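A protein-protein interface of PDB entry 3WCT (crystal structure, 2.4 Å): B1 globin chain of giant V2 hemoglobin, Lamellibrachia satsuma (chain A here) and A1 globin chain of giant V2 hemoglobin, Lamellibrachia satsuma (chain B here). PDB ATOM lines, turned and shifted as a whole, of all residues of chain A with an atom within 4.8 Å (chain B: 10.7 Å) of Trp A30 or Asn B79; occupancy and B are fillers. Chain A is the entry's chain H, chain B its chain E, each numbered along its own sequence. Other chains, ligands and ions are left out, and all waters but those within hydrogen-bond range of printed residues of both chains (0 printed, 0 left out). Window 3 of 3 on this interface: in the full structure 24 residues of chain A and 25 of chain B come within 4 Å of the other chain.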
ATOM      1  N   ALA A  26      28.856  18.849  21.018  1.00  0.00           N
ATOM      2  CA  ALA A  26      28.819  18.254  19.684  1.00  0.00           C
ATOM      3  C   ALA A  26      29.022  19.273  18.559  1.00  0.00           C
ATOM      4  O   ALA A  26      29.745  19.008  17.593  1.00  0.00           O
ATOM      5  CB  ALA A  26      27.509  17.519  19.487  1.00  0.00           C
ATOM      6  N   LYS A  27      28.392  20.438  18.688  1.00  0.00           N
ATOM      7  CA  LYS A  27      28.506  21.474  17.669  1.00  0.00           C
ATOM      8  C   LYS A  27      29.954  21.815  17.311  1.00  0.00           C
ATOM      9  O   LYS A  27      30.311  21.855  16.125  1.00  0.00           O
ATOM     10  CB  LYS A  27      27.777  22.750  18.098  1.00  0.00           C
ATOM     11  CG  LYS A  27      27.750  23.823  16.999  1.00  0.00           C
ATOM     12  CD  LYS A  27      26.885  25.010  17.380  1.00  0.00           C
ATOM     13  CE  LYS A  27      26.659  25.923  16.185  1.00  0.00           C
ATOM     14  NZ  LYS A  27      25.690  27.019  16.511  1.00  0.00           N
ATOM     15  N   SER A  28      30.776  22.071  18.329  1.00  0.00           N
ATOM     16  CA  SER A  28      32.181  22.397  18.116  1.00  0.00           C
ATOM     17  C   SER A  28      32.807  21.206  17.413  1.00  0.00           C
ATOM     18  O   SER A  28      33.642  21.358  16.529  1.00  0.00           O
ATOM     19  CB  SER A  28      32.913  22.591  19.450  1.00  0.00           C
ATOM     20  OG  SER A  28      32.037  23.059  20.455  1.00  0.00           O
ATOM     21  N   ARG A  29      32.394  20.016  17.836  1.00  0.00           N
ATOM     22  CA  ARG A  29      32.912  18.789  17.275  1.00  0.00           C
ATOM     23  C   ARG A  29      32.650  18.643  15.781  1.00  0.00           C
ATOM     24  O   ARG A  29      33.597  18.431  15.016  1.00  0.00           O
ATOM     25  CB  ARG A  29      32.364  17.580  18.038  1.00  0.00           C
ATOM     26  CG  ARG A  29      32.828  17.529  19.488  1.00  0.00           C
ATOM     27  CD  ARG A  29      32.479  16.201  20.135  1.00  0.00           C
ATOM     28  NE  ARG A  29      32.443  16.285  21.590  1.00  0.00           N
ATOM     29  CZ  ARG A  29      32.435  15.226  22.396  1.00  0.00           C
ATOM     30  NH1 ARG A  29      32.396  15.389  23.711  1.00  0.00           N
ATOM     31  NH2 ARG A  29      32.484  14.000  21.888  1.00  0.00           N
ATOM     32  N   TRP A  30      31.400  18.764  15.338  1.00  0.00           N
ATOM     33  CA  TRP A  30      31.176  18.614  13.901  1.00  0.00           C
ATOM     34  C   TRP A  30      31.692  19.839  13.159  1.00  0.00           C
ATOM     35  O   TRP A  30      31.883  19.804  11.942  1.00  0.00           O
ATOM     36  CB  TRP A  30      29.698  18.324  13.560  1.00  0.00           C
ATOM     37  CG  TRP A  30      28.709  19.417  13.813  1.00  0.00           C
ATOM     38  CD1 TRP A  30      28.687  20.661  13.244  1.00  0.00           C
ATOM     39  CD2 TRP A  30      27.558  19.345  14.663  1.00  0.00           C
ATOM     40  NE1 TRP A  30      27.590  21.364  13.685  1.00  0.00           N
ATOM     41  CE2 TRP A  30      26.881  20.580  14.557  1.00  0.00           C
ATOM     42  CE3 TRP A  30      27.033  18.356  15.502  1.00  0.00           C
ATOM     43  CZ2 TRP A  30      25.700  20.852  15.263  1.00  0.00           C
ATOM     44  CZ3 TRP A  30      25.859  18.627  16.204  1.00  0.00           C
ATOM     45  CH2 TRP A  30      25.207  19.865  16.079  1.00  0.00           C
ATOM     46  N   THR A  31      31.939  20.920  13.893  1.00  0.00           N
ATOM     47  CA  THR A  31      32.476  22.112  13.263  1.00  0.00           C
ATOM     48  C   THR A  31      33.911  21.798  12.868  1.00  0.00           C
ATOM     49  O   THR A  31      34.338  22.131  11.770  1.00  0.00           O
ATOM     50  CB  THR A  31      32.448  23.318  14.200  1.00  0.00           C
ATOM     51  OG1 THR A  31      31.092  23.622  14.518  1.00  0.00           O
ATOM     52  CG2 THR A  31      33.076  24.535  13.536  1.00  0.00           C
ATOM     53  N   MET A  32      34.656  21.147  13.754  1.00  0.00           N
ATOM     54  CA  MET A  32      36.033  20.779  13.423  1.00  0.00           C
ATOM     55  C   MET A  32      35.945  19.689  12.356  1.00  0.00           C
ATOM     56  O   MET A  32      36.763  19.620  11.434  1.00  0.00           O
ATOM     57  CB  MET A  32      36.756  20.223  14.646  1.00  0.00           C
ATOM     58  CG  MET A  32      36.984  21.221  15.763  1.00  0.00           C
ATOM     59  SD  MET A  32      37.471  20.355  17.267  1.00  0.00           S
ATOM     60  CE  MET A  32      39.136  20.016  16.917  1.00  0.00           C
ATOM     61  N   GLY A  33      34.935  18.836  12.500  1.00  0.00           N
ATOM     62  CA  GLY A  33      34.734  17.760  11.546  1.00  0.00           C
ATOM     63  C   GLY A  33      34.559  18.274  10.125  1.00  0.00           C
ATOM     64  O   GLY A  33      35.252  17.824   9.209  1.00  0.00           O
ATOM     65  N   ASN A  34      33.639  19.217   9.941  1.00  0.00           N
ATOM     66  CA  ASN A  34      33.388  19.781   8.619  1.00  0.00           C
ATOM     67  C   ASN A  34      34.616  20.448   7.991  1.00  0.00           C
ATOM     68  O   ASN A  34      34.879  20.257   6.800  1.00  0.00           O
ATOM     69  CB  ASN A  34      32.215  20.764   8.681  1.00  0.00           C
ATOM     70  CG  ASN A  34      30.866  20.062   8.604  1.00  0.00           C
ATOM     71  OD1 ASN A  34      30.729  18.893   8.988  1.00  0.00           O
ATOM     72  ND2 ASN A  34      29.859  20.777   8.114  1.00  0.00           N
ATOM     73  N   HIS A  65      26.865  14.993  10.369  1.00  0.00           N
ATOM     74  CA  HIS A  65      27.382  15.506  11.631  1.00  0.00           C
ATOM     75  C   HIS A  65      27.783  14.316  12.492  1.00  0.00           C
ATOM     76  O   HIS A  65      28.893  14.278  13.024  1.00  0.00           O
ATOM     77  CB  HIS A  65      26.332  16.357  12.355  1.00  0.00           C
ATOM     78  CG  HIS A  65      26.268  17.770  11.865  1.00  0.00           C
ATOM     79  ND1 HIS A  65      25.287  18.651  12.261  1.00  0.00           N
ATOM     80  CD2 HIS A  65      27.070  18.456  11.016  1.00  0.00           C
ATOM     81  CE1 HIS A  65      25.485  19.820  11.675  1.00  0.00           C
ATOM     82  NE2 HIS A  65      26.560  19.728  10.915  1.00  0.00           N
ATOM     83  N   THR A  68      31.150  12.739  11.253  1.00  0.00           N
ATOM     84  CA  THR A  68      32.367  13.411  11.703  1.00  0.00           C
ATOM     85  C   THR A  68      32.583  13.237  13.211  1.00  0.00           C
ATOM     86  O   THR A  68      33.718  13.129  13.675  1.00  0.00           O
ATOM     87  CB  THR A  68      32.336  14.910  11.385  1.00  0.00           C
ATOM     88  OG1 THR A  68      31.136  15.483  11.917  1.00  0.00           O
ATOM     89  CG2 THR A  68      32.400  15.137   9.883  1.00  0.00           C
ATOM     90  N   VAL A  69      31.490  13.194  13.966  1.00  0.00           N
ATOM     91  CA  VAL A  69      31.582  13.036  15.402  1.00  0.00           C
ATOM     92  C   VAL A  69      32.199  11.691  15.749  1.00  0.00           C
ATOM     93  O   VAL A  69      33.133  11.634  16.551  1.00  0.00           O
ATOM     94  CB  VAL A  69      30.188  13.206  16.077  1.00  0.00           C
ATOM     95  CG1 VAL A  69      30.215  12.699  17.518  1.00  0.00           C
ATOM     96  CG2 VAL A  69      29.802  14.675  16.073  1.00  0.00           C
ATOM     97  N   CYS B   2      12.915  13.237  29.509  1.00  0.00           N
ATOM     98  CA  CYS B   2      14.231  13.679  29.052  1.00  0.00           C
ATOM     99  C   CYS B   2      14.129  14.936  28.191  1.00  0.00           C
ATOM    100  O   CYS B   2      14.503  14.951  27.013  1.00  0.00           O
ATOM    101  CB  CYS B   2      14.979  12.568  28.288  1.00  0.00           C
ATOM    102  SG  CYS B   2      16.656  13.099  27.796  1.00  0.00           S
ATOM    103  N   ASN B   3      13.604  15.994  28.800  1.00  0.00           N
ATOM    104  CA  ASN B   3      13.469  17.269  28.127  1.00  0.00           C
ATOM    105  C   ASN B   3      14.867  17.872  27.989  1.00  0.00           C
ATOM    106  O   ASN B   3      15.858  17.261  28.376  1.00  0.00           O
ATOM    107  CB  ASN B   3      12.544  18.194  28.929  1.00  0.00           C
ATOM    108  CG  ASN B   3      13.015  18.410  30.363  1.00  0.00           C
ATOM    109  OD1 ASN B   3      14.077  18.988  30.600  1.00  0.00           O
ATOM    110  ND2 ASN B   3      12.217  17.948  31.329  1.00  0.00           N
ATOM    111  N   ILE B   4      14.943  19.073  27.443  1.00  0.00           N
ATOM    112  CA  ILE B   4      16.219  19.736  27.244  1.00  0.00           C
ATOM    113  C   ILE B   4      16.993  19.994  28.539  1.00  0.00           C
ATOM    114  O   ILE B   4      18.216  19.865  28.570  1.00  0.00           O
ATOM    115  CB  ILE B   4      16.024  21.074  26.500  1.00  0.00           C
ATOM    116  CG1 ILE B   4      17.369  21.600  26.013  1.00  0.00           C
ATOM    117  CG2 ILE B   4      15.366  22.097  27.419  1.00  0.00           C
ATOM    118  CD1 ILE B   4      17.255  22.873  25.222  1.00  0.00           C
ATOM    119  N   ARG B   7      18.701  16.853  29.624  1.00  0.00           N
ATOM    120  CA  ARG B   7      19.791  16.531  28.703  1.00  0.00           C
ATOM    121  C   ARG B   7      21.039  17.321  29.081  1.00  0.00           C
ATOM    122  O   ARG B   7      22.144  16.775  29.073  1.00  0.00           O
ATOM    123  CB  ARG B   7      19.383  16.839  27.254  1.00  0.00           C
ATOM    124  CG  ARG B   7      18.291  15.917  26.762  1.00  0.00           C
ATOM    125  CD  ARG B   7      17.731  16.257  25.397  1.00  0.00           C
ATOM    126  NE  ARG B   7      16.620  15.351  25.126  1.00  0.00           N
ATOM    127  CZ  ARG B   7      16.538  14.547  24.070  1.00  0.00           C
ATOM    128  NH1 ARG B   7      17.497  14.533  23.152  1.00  0.00           N
ATOM    129  NH2 ARG B   7      15.510  13.716  23.959  1.00  0.00           N
ATOM    130  N   LEU B   8      20.846  18.595  29.426  1.00  0.00           N
ATOM    131  CA  LEU B   8      21.951  19.467  29.826  1.00  0.00           C
ATOM    132  C   LEU B   8      22.581  19.029  31.153  1.00  0.00           C
ATOM    133  O   LEU B   8      23.802  18.996  31.276  1.00  0.00           O
ATOM    134  CB  LEU B   8      21.476  20.924  29.929  1.00  0.00           C
ATOM    135  CG  LEU B   8      21.040  21.580  28.608  1.00  0.00           C
ATOM    136  CD1 LEU B   8      20.514  22.991  28.873  1.00  0.00           C
ATOM    137  CD2 LEU B   8      22.225  21.622  27.618  1.00  0.00           C
ATOM    138  N   LYS B  11      24.601  15.991  30.461  1.00  0.00           N
ATOM    139  CA  LYS B  11      25.840  16.228  29.731  1.00  0.00           C
ATOM    140  C   LYS B  11      26.876  16.752  30.731  1.00  0.00           C
ATOM    141  O   LYS B  11      28.048  16.373  30.697  1.00  0.00           O
ATOM    142  CB  LYS B  11      25.617  17.255  28.610  1.00  0.00           C
ATOM    143  CG  LYS B  11      24.996  16.670  27.347  1.00  0.00           C
ATOM    144  CD  LYS B  11      24.225  17.706  26.514  1.00  0.00           C
ATOM    145  CE  LYS B  11      25.126  18.801  25.968  1.00  0.00           C
ATOM    146  NZ  LYS B  11      26.179  18.253  25.070  1.00  0.00           N
ATOM    147  N   ARG B  72      30.219  10.498  22.657  1.00  0.00           N
ATOM    148  CA  ARG B  72      29.728  11.194  21.473  1.00  0.00           C
ATOM    149  C   ARG B  72      28.201  11.265  21.503  1.00  0.00           C
ATOM    150  O   ARG B  72      27.615  12.290  21.165  1.00  0.00           O
ATOM    151  CB  ARG B  72      30.220  10.498  20.198  1.00  0.00           C
ATOM    152  CG  ARG B  72      29.710   9.079  20.014  1.00  0.00           C
ATOM    153  CD  ARG B  72      30.378   8.390  18.821  1.00  0.00           C
ATOM    154  NE  ARG B  72      29.409   7.564  18.104  1.00  0.00           N
ATOM    155  CZ  ARG B  72      29.600   6.305  17.720  1.00  0.00           C
ATOM    156  NH1 ARG B  72      30.745   5.677  17.968  1.00  0.00           N
ATOM    157  NH2 ARG B  72      28.620   5.666  17.098  1.00  0.00           N
ATOM    158  N   VAL B  73      27.561  10.187  21.946  1.00  0.00           N
ATOM    159  CA  VAL B  73      26.105  10.158  22.013  1.00  0.00           C
ATOM    160  C   VAL B  73      25.583  11.191  23.010  1.00  0.00           C
ATOM    161  O   VAL B  73      24.622  11.914  22.727  1.00  0.00           O
ATOM    162  CB  VAL B  73      25.599   8.752  22.401  1.00  0.00           C
ATOM    163  CG1 VAL B  73      24.109   8.791  22.703  1.00  0.00           C
ATOM    164  CG2 VAL B  73      25.881   7.778  21.265  1.00  0.00           C
ATOM    165  N   ILE B  74      26.223  11.269  24.172  1.00  0.00           N
ATOM    166  CA  ILE B  74      25.812  12.222  25.189  1.00  0.00           C
ATOM    167  C   ILE B  74      26.092  13.669  24.756  1.00  0.00           C
ATOM    168  O   ILE B  74      25.346  14.587  25.115  1.00  0.00           O
ATOM    169  CB  ILE B  74      26.506  11.901  26.545  1.00  0.00           C
ATOM    170  CG1 ILE B  74      25.741  10.779  27.258  1.00  0.00           C
ATOM    171  CG2 ILE B  74      26.577  13.144  27.415  1.00  0.00           C
ATOM    172  CD1 ILE B  74      26.418  10.257  28.525  1.00  0.00           C
ATOM    173  N   SER B  75      27.148  13.863  23.968  1.00  0.00           N
ATOM    174  CA  SER B  75      27.510  15.193  23.497  1.00  0.00           C
ATOM    175  C   SER B  75      26.540  15.707  22.437  1.00  0.00           C
ATOM    176  O   SER B  75      26.471  16.912  22.186  1.00  0.00           O
ATOM    177  CB  SER B  75      28.925  15.193  22.920  1.00  0.00           C
ATOM    178  OG  SER B  75      28.937  14.666  21.605  1.00  0.00           O
ATOM    179  N   MET B  76      25.795  14.797  21.814  1.00  0.00           N
ATOM    180  CA  MET B  76      24.838  15.184  20.781  1.00  0.00           C
ATOM    181  C   MET B  76      23.428  15.293  21.346  1.00  0.00           C
ATOM    182  O   MET B  76      22.489  15.588  20.612  1.00  0.00           O
ATOM    183  CB  MET B  76      24.846  14.174  19.623  1.00  0.00           C
ATOM    184  CG  MET B  76      26.102  14.197  18.739  1.00  0.00           C
ATOM    185  SD  MET B  76      26.067  12.945  17.387  1.00  0.00           S
ATOM    186  CE  MET B  76      26.578  11.450  18.287  1.00  0.00           C
ATOM    187  N   PHE B  77      23.278  15.066  22.648  1.00  0.00           N
ATOM    188  CA  PHE B  77      21.961  15.124  23.276  1.00  0.00           C
ATOM    189  C   PHE B  77      21.150  16.363  22.906  1.00  0.00           C
ATOM    190  O   PHE B  77      19.919  16.335  22.893  1.00  0.00           O
ATOM    191  CB  PHE B  77      22.085  15.064  24.801  1.00  0.00           C
ATOM    192  CG  PHE B  77      21.715  13.732  25.396  1.00  0.00           C
ATOM    193  CD1 PHE B  77      20.868  12.857  24.726  1.00  0.00           C
ATOM    194  CD2 PHE B  77      22.183  13.368  26.657  1.00  0.00           C
ATOM    195  CE1 PHE B  77      20.495  11.644  25.300  1.00  0.00           C
ATOM    196  CE2 PHE B  77      21.815  12.154  27.243  1.00  0.00           C
ATOM    197  CZ  PHE B  77      20.970  11.293  26.566  1.00  0.00           C
ATOM    198  N   ASP B  78      21.852  17.447  22.606  1.00  0.00           N
ATOM    199  CA  ASP B  78      21.222  18.718  22.283  1.00  0.00           C
ATOM    200  C   ASP B  78      20.843  18.912  20.815  1.00  0.00           C
ATOM    201  O   ASP B  78      20.220  19.916  20.464  1.00  0.00           O
ATOM    202  CB  ASP B  78      22.144  19.856  22.733  1.00  0.00           C
ATOM    203  CG  ASP B  78      23.606  19.582  22.397  1.00  0.00           C
ATOM    204  OD1 ASP B  78      23.890  19.120  21.266  1.00  0.00           O
ATOM    205  OD2 ASP B  78      24.476  19.833  23.264  1.00  0.00           O
ATOM    206  N   ASN B  79      21.223  17.972  19.956  1.00  0.00           N
ATOM    207  CA  ASN B  79      20.888  18.087  18.541  1.00  0.00           C
ATOM    208  C   ASN B  79      20.236  16.816  18.013  1.00  0.00           C
ATOM    209  O   ASN B  79      20.914  15.879  17.578  1.00  0.00           O
ATOM    210  CB  ASN B  79      22.127  18.420  17.703  1.00  0.00           C
ATOM    211  CG  ASN B  79      21.793  18.597  16.231  1.00  0.00           C
ATOM    212  OD1 ASN B  79      21.522  17.628  15.526  1.00  0.00           O
ATOM    213  ND2 ASN B  79      21.790  19.840  15.768  1.00  0.00           N
ATOM    214  N   GLU B  80      18.906  16.813  18.055  1.00  0.00           N
ATOM    215  CA  GLU B  80      18.088  15.692  17.614  1.00  0.00           C
ATOM    216  C   GLU B  80      18.508  14.998  16.325  1.00  0.00           C
ATOM    217  O   GLU B  80      18.583  13.772  16.289  1.00  0.00           O
ATOM    218  CB  GLU B  80      16.635  16.148  17.496  1.00  0.00           C
ATOM    219  CG  GLU B  80      15.868  16.104  18.802  1.00  0.00           C
ATOM    220  CD  GLU B  80      15.463  14.690  19.175  1.00  0.00           C
ATOM    221  OE1 GLU B  80      15.984  14.147  20.177  1.00  0.00           O
ATOM    222  OE2 GLU B  80      14.621  14.116  18.449  1.00  0.00           O
ATOM    223  N   ASP B  81      18.774  15.764  15.269  1.00  0.00           N
ATOM    224  CA  ASP B  81      19.155  15.158  13.992  1.00  0.00           C
ATOM    225  C   ASP B  81      20.443  14.339  14.093  1.00  0.00           C
ATOM    226  O   ASP B  81      20.497  13.198  13.631  1.00  0.00           O
ATOM    227  CB  ASP B  81      19.302  16.224  12.887  1.00  0.00           C
ATOM    228  CG  ASP B  81      17.960  16.856  12.484  1.00  0.00           C
ATOM    229  OD1 ASP B  81      16.965  16.114  12.320  1.00  0.00           O
ATOM    230  OD2 ASP B  81      17.905  18.099  12.319  1.00  0.00           O
ATOM    231  N   ALA B  82      21.473  14.922  14.697  1.00  0.00           N
ATOM    232  CA  ALA B  82      22.749  14.236  14.851  1.00  0.00           C
ATOM    233  C   ALA B  82      22.565  13.042  15.779  1.00  0.00           C
ATOM    234  O   ALA B  82      23.043  11.945  15.503  1.00  0.00           O
ATOM    235  CB  ALA B  82      23.787  15.192  15.419  1.00  0.00           C
ATOM    236  N   LEU B  83      21.855  13.264  16.876  1.00  0.00           N
ATOM    237  CA  LEU B  83      21.608  12.217  17.847  1.00  0.00           C
ATOM    238  C   LEU B  83      20.960  10.996  17.221  1.00  0.00           C
ATOM    239  O   LEU B  83      21.476   9.883  17.338  1.00  0.00           O
ATOM    240  CB  LEU B  83      20.716  12.741  18.976  1.00  0.00           C
ATOM    241  CG  LEU B  83      20.271  11.731  20.039  1.00  0.00           C
ATOM    242  CD1 LEU B  83      21.491  11.105  20.700  1.00  0.00           C
ATOM    243  CD2 LEU B  83      19.389  12.428  21.073  1.00  0.00           C
ATOM    244  N   ASN B  84      19.829  11.191  16.554  1.00  0.00           N
ATOM    245  CA  ASN B  84      19.130  10.057  15.958  1.00  0.00           C
ATOM    246  C   ASN B  84      19.922   9.315  14.889  1.00  0.00           C
ATOM    247  O   ASN B  84      19.798   8.104  14.751  1.00  0.00           O
ATOM    248  CB  ASN B  84      17.767  10.500  15.422  1.00  0.00           C
ATOM    249  CG  ASN B  84      16.786  10.818  16.548  1.00  0.00           C
ATOM    250  OD1 ASN B  84      16.657  10.047  17.499  1.00  0.00           O
ATOM    251  ND2 ASN B  84      16.097  11.949  16.448  1.00  0.00           N
ATOM    252  N   ALA B  85      20.757  10.030  14.149  1.00  0.00           N
ATOM    253  CA  ALA B  85      21.551   9.392  13.115  1.00  0.00           C
ATOM    254  C   ALA B  85      22.559   8.426  13.728  1.00  0.00           C
ATOM    255  O   ALA B  85      22.717   7.297  13.257  1.00  0.00           O
ATOM    256  CB  ALA B  85      22.269  10.449  12.275  1.00  0.00           C
ATOM    257  N   ASP B  86      23.232   8.866  14.788  1.00  0.00           N
ATOM    258  CA  ASP B  86      24.235   8.034  15.441  1.00  0.00           C
ATOM    259  C   ASP B  86      23.622   6.867  16.203  1.00  0.00           C
ATOM    260  O   ASP B  86      24.209   5.790  16.261  1.00  0.00           O
ATOM    261  CB  ASP B  86      25.111   8.887  16.364  1.00  0.00           C
ATOM    262  CG  ASP B  86      26.465   8.256  16.623  1.00  0.00           C
ATOM    263  OD1 ASP B  86      27.044   7.670  15.683  1.00  0.00           O
ATOM    264  OD2 ASP B  86      26.957   8.354  17.764  1.00  0.00           O
ATOM    265  N   LEU B  87      22.445   7.070  16.784  1.00  0.00           N
ATOM    266  CA  LEU B  87      21.775   5.984  17.497  1.00  0.00           C
ATOM    267  C   LEU B  87      21.374   4.895  16.489  1.00  0.00           C
ATOM    268  O   LEU B  87      21.401   3.699  16.801  1.00  0.00           O
ATOM    269  CB  LEU B  87      20.535   6.504  18.227  1.00  0.00           C
ATOM    270  CG  LEU B  87      20.818   7.284  19.516  1.00  0.00           C
ATOM    271  CD1 LEU B  87      19.540   7.919  20.037  1.00  0.00           C
ATOM    272  CD2 LEU B  87      21.414   6.348  20.545  1.00  0.00           C
ATOM    273  N   VAL B 134      16.284   7.142  26.124  1.00  0.00           N
ATOM    274  CA  VAL B 134      16.363   7.614  24.749  1.00  0.00           C
ATOM    275  C   VAL B 134      17.477   6.875  23.996  1.00  0.00           C
ATOM    276  O   VAL B 134      17.304   6.481  22.845  1.00  0.00           O
ATOM    277  CB  VAL B 134      16.624   9.140  24.693  1.00  0.00           C
ATOM    278  CG1 VAL B 134      16.859   9.583  23.258  1.00  0.00           C
ATOM    279  CG2 VAL B 134      15.434   9.888  25.266  1.00  0.00           C
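Along chain B the printed residues that touch a printed residue of chain A span positions 72 to 79. Printed residues of chain A that touch a printed residue of chain B: Ala A26, Arg A29, Trp A30 and Val A69. Hydrophobic or aromatic side chains of chain A within 4 Å of the printed part of chain B: Ala A26, Trp A30 and Val A69. Among the printed residues, no Asp or Glu carboxylate lies within 4 Å of a Lys or Arg side-chain nitrogen of the other chain.
The side-chain amino group (NZ) of Lys B11 lies within hydrogen-bond range of the backbone carbonyl oxygen (O) of Ser B75 (3.2 Å). The side-chain hydroxyl of Ser B75 lies within hydrogen-bond range of the backbone carbonyl oxygen of Arg B72, 2.8 Å away. The guanidinium group (NE) of Arg B72 lies within salt-bridge range of the side-chain carboxylate (OD2) of Asp B86 (2.6 Å). The side-chain amide oxygen (OD1) of Asn B79 sits close to the backbone NH (N) of Asp B81 (3.3 Å). The side-chain amide oxygen (OD1) of Asn B79 is in hydrogen-bond range of the backbone NH (N) of Ala B82 (2.8 Å). The side-chain amide oxygen (OD1) of Asn A34 lies close to the backbone carbonyl oxygen (O) of Trp A30 (3.3 Å).
The backbone carbonyl oxygen (O) of Ser B75 lies close to the backbone NH (N) of Ala A26 (3.3 Å).
Ala A26 touches Met B76. NH2 of Arg A29 touches CA of Arg B72, 3.95 Å away. Ser B75 touches Arg A29 (CB to CZ, 3.5 Å). Trp A30 touches Asn B79 (CH2 to ND2, 3.4 Å). Arg B72 touches Val A69 (CB to CG1, 3.5 Å). Val A69 touches Met B76.
No residue of chain B comes within 4 Å of Lys A27. Of the printed residues of chain B, Arg A29 touches Arg B72 (3.95 Å) and Ser B75 (3.5 Å). No residue of chain B comes within 4 Å of Gly A33. No residue of chain B comes within 4 Å of Thr A68. Printed residues of chain B within 4 Å of Val A69: Arg B72 and Met B76. Printed residues of chain A within 4 Å of Arg B72: Arg A29 and Val A69. Of the printed residues of chain A, Ser B75 touches Ala A26 (3.0 Å) and Arg A29 (3.5 Å). Printed residues of chain A within 4 Å of Met B76: Ala A26 and Val A69. Asn B79 touches one residue of chain A. The nearest printed residue of chain A that does not touch Asn B79 is His A65 (5.1 Å). The nearest printed residue of chain B that does not touch Arg A29 is Val B73 (6.2 Å).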
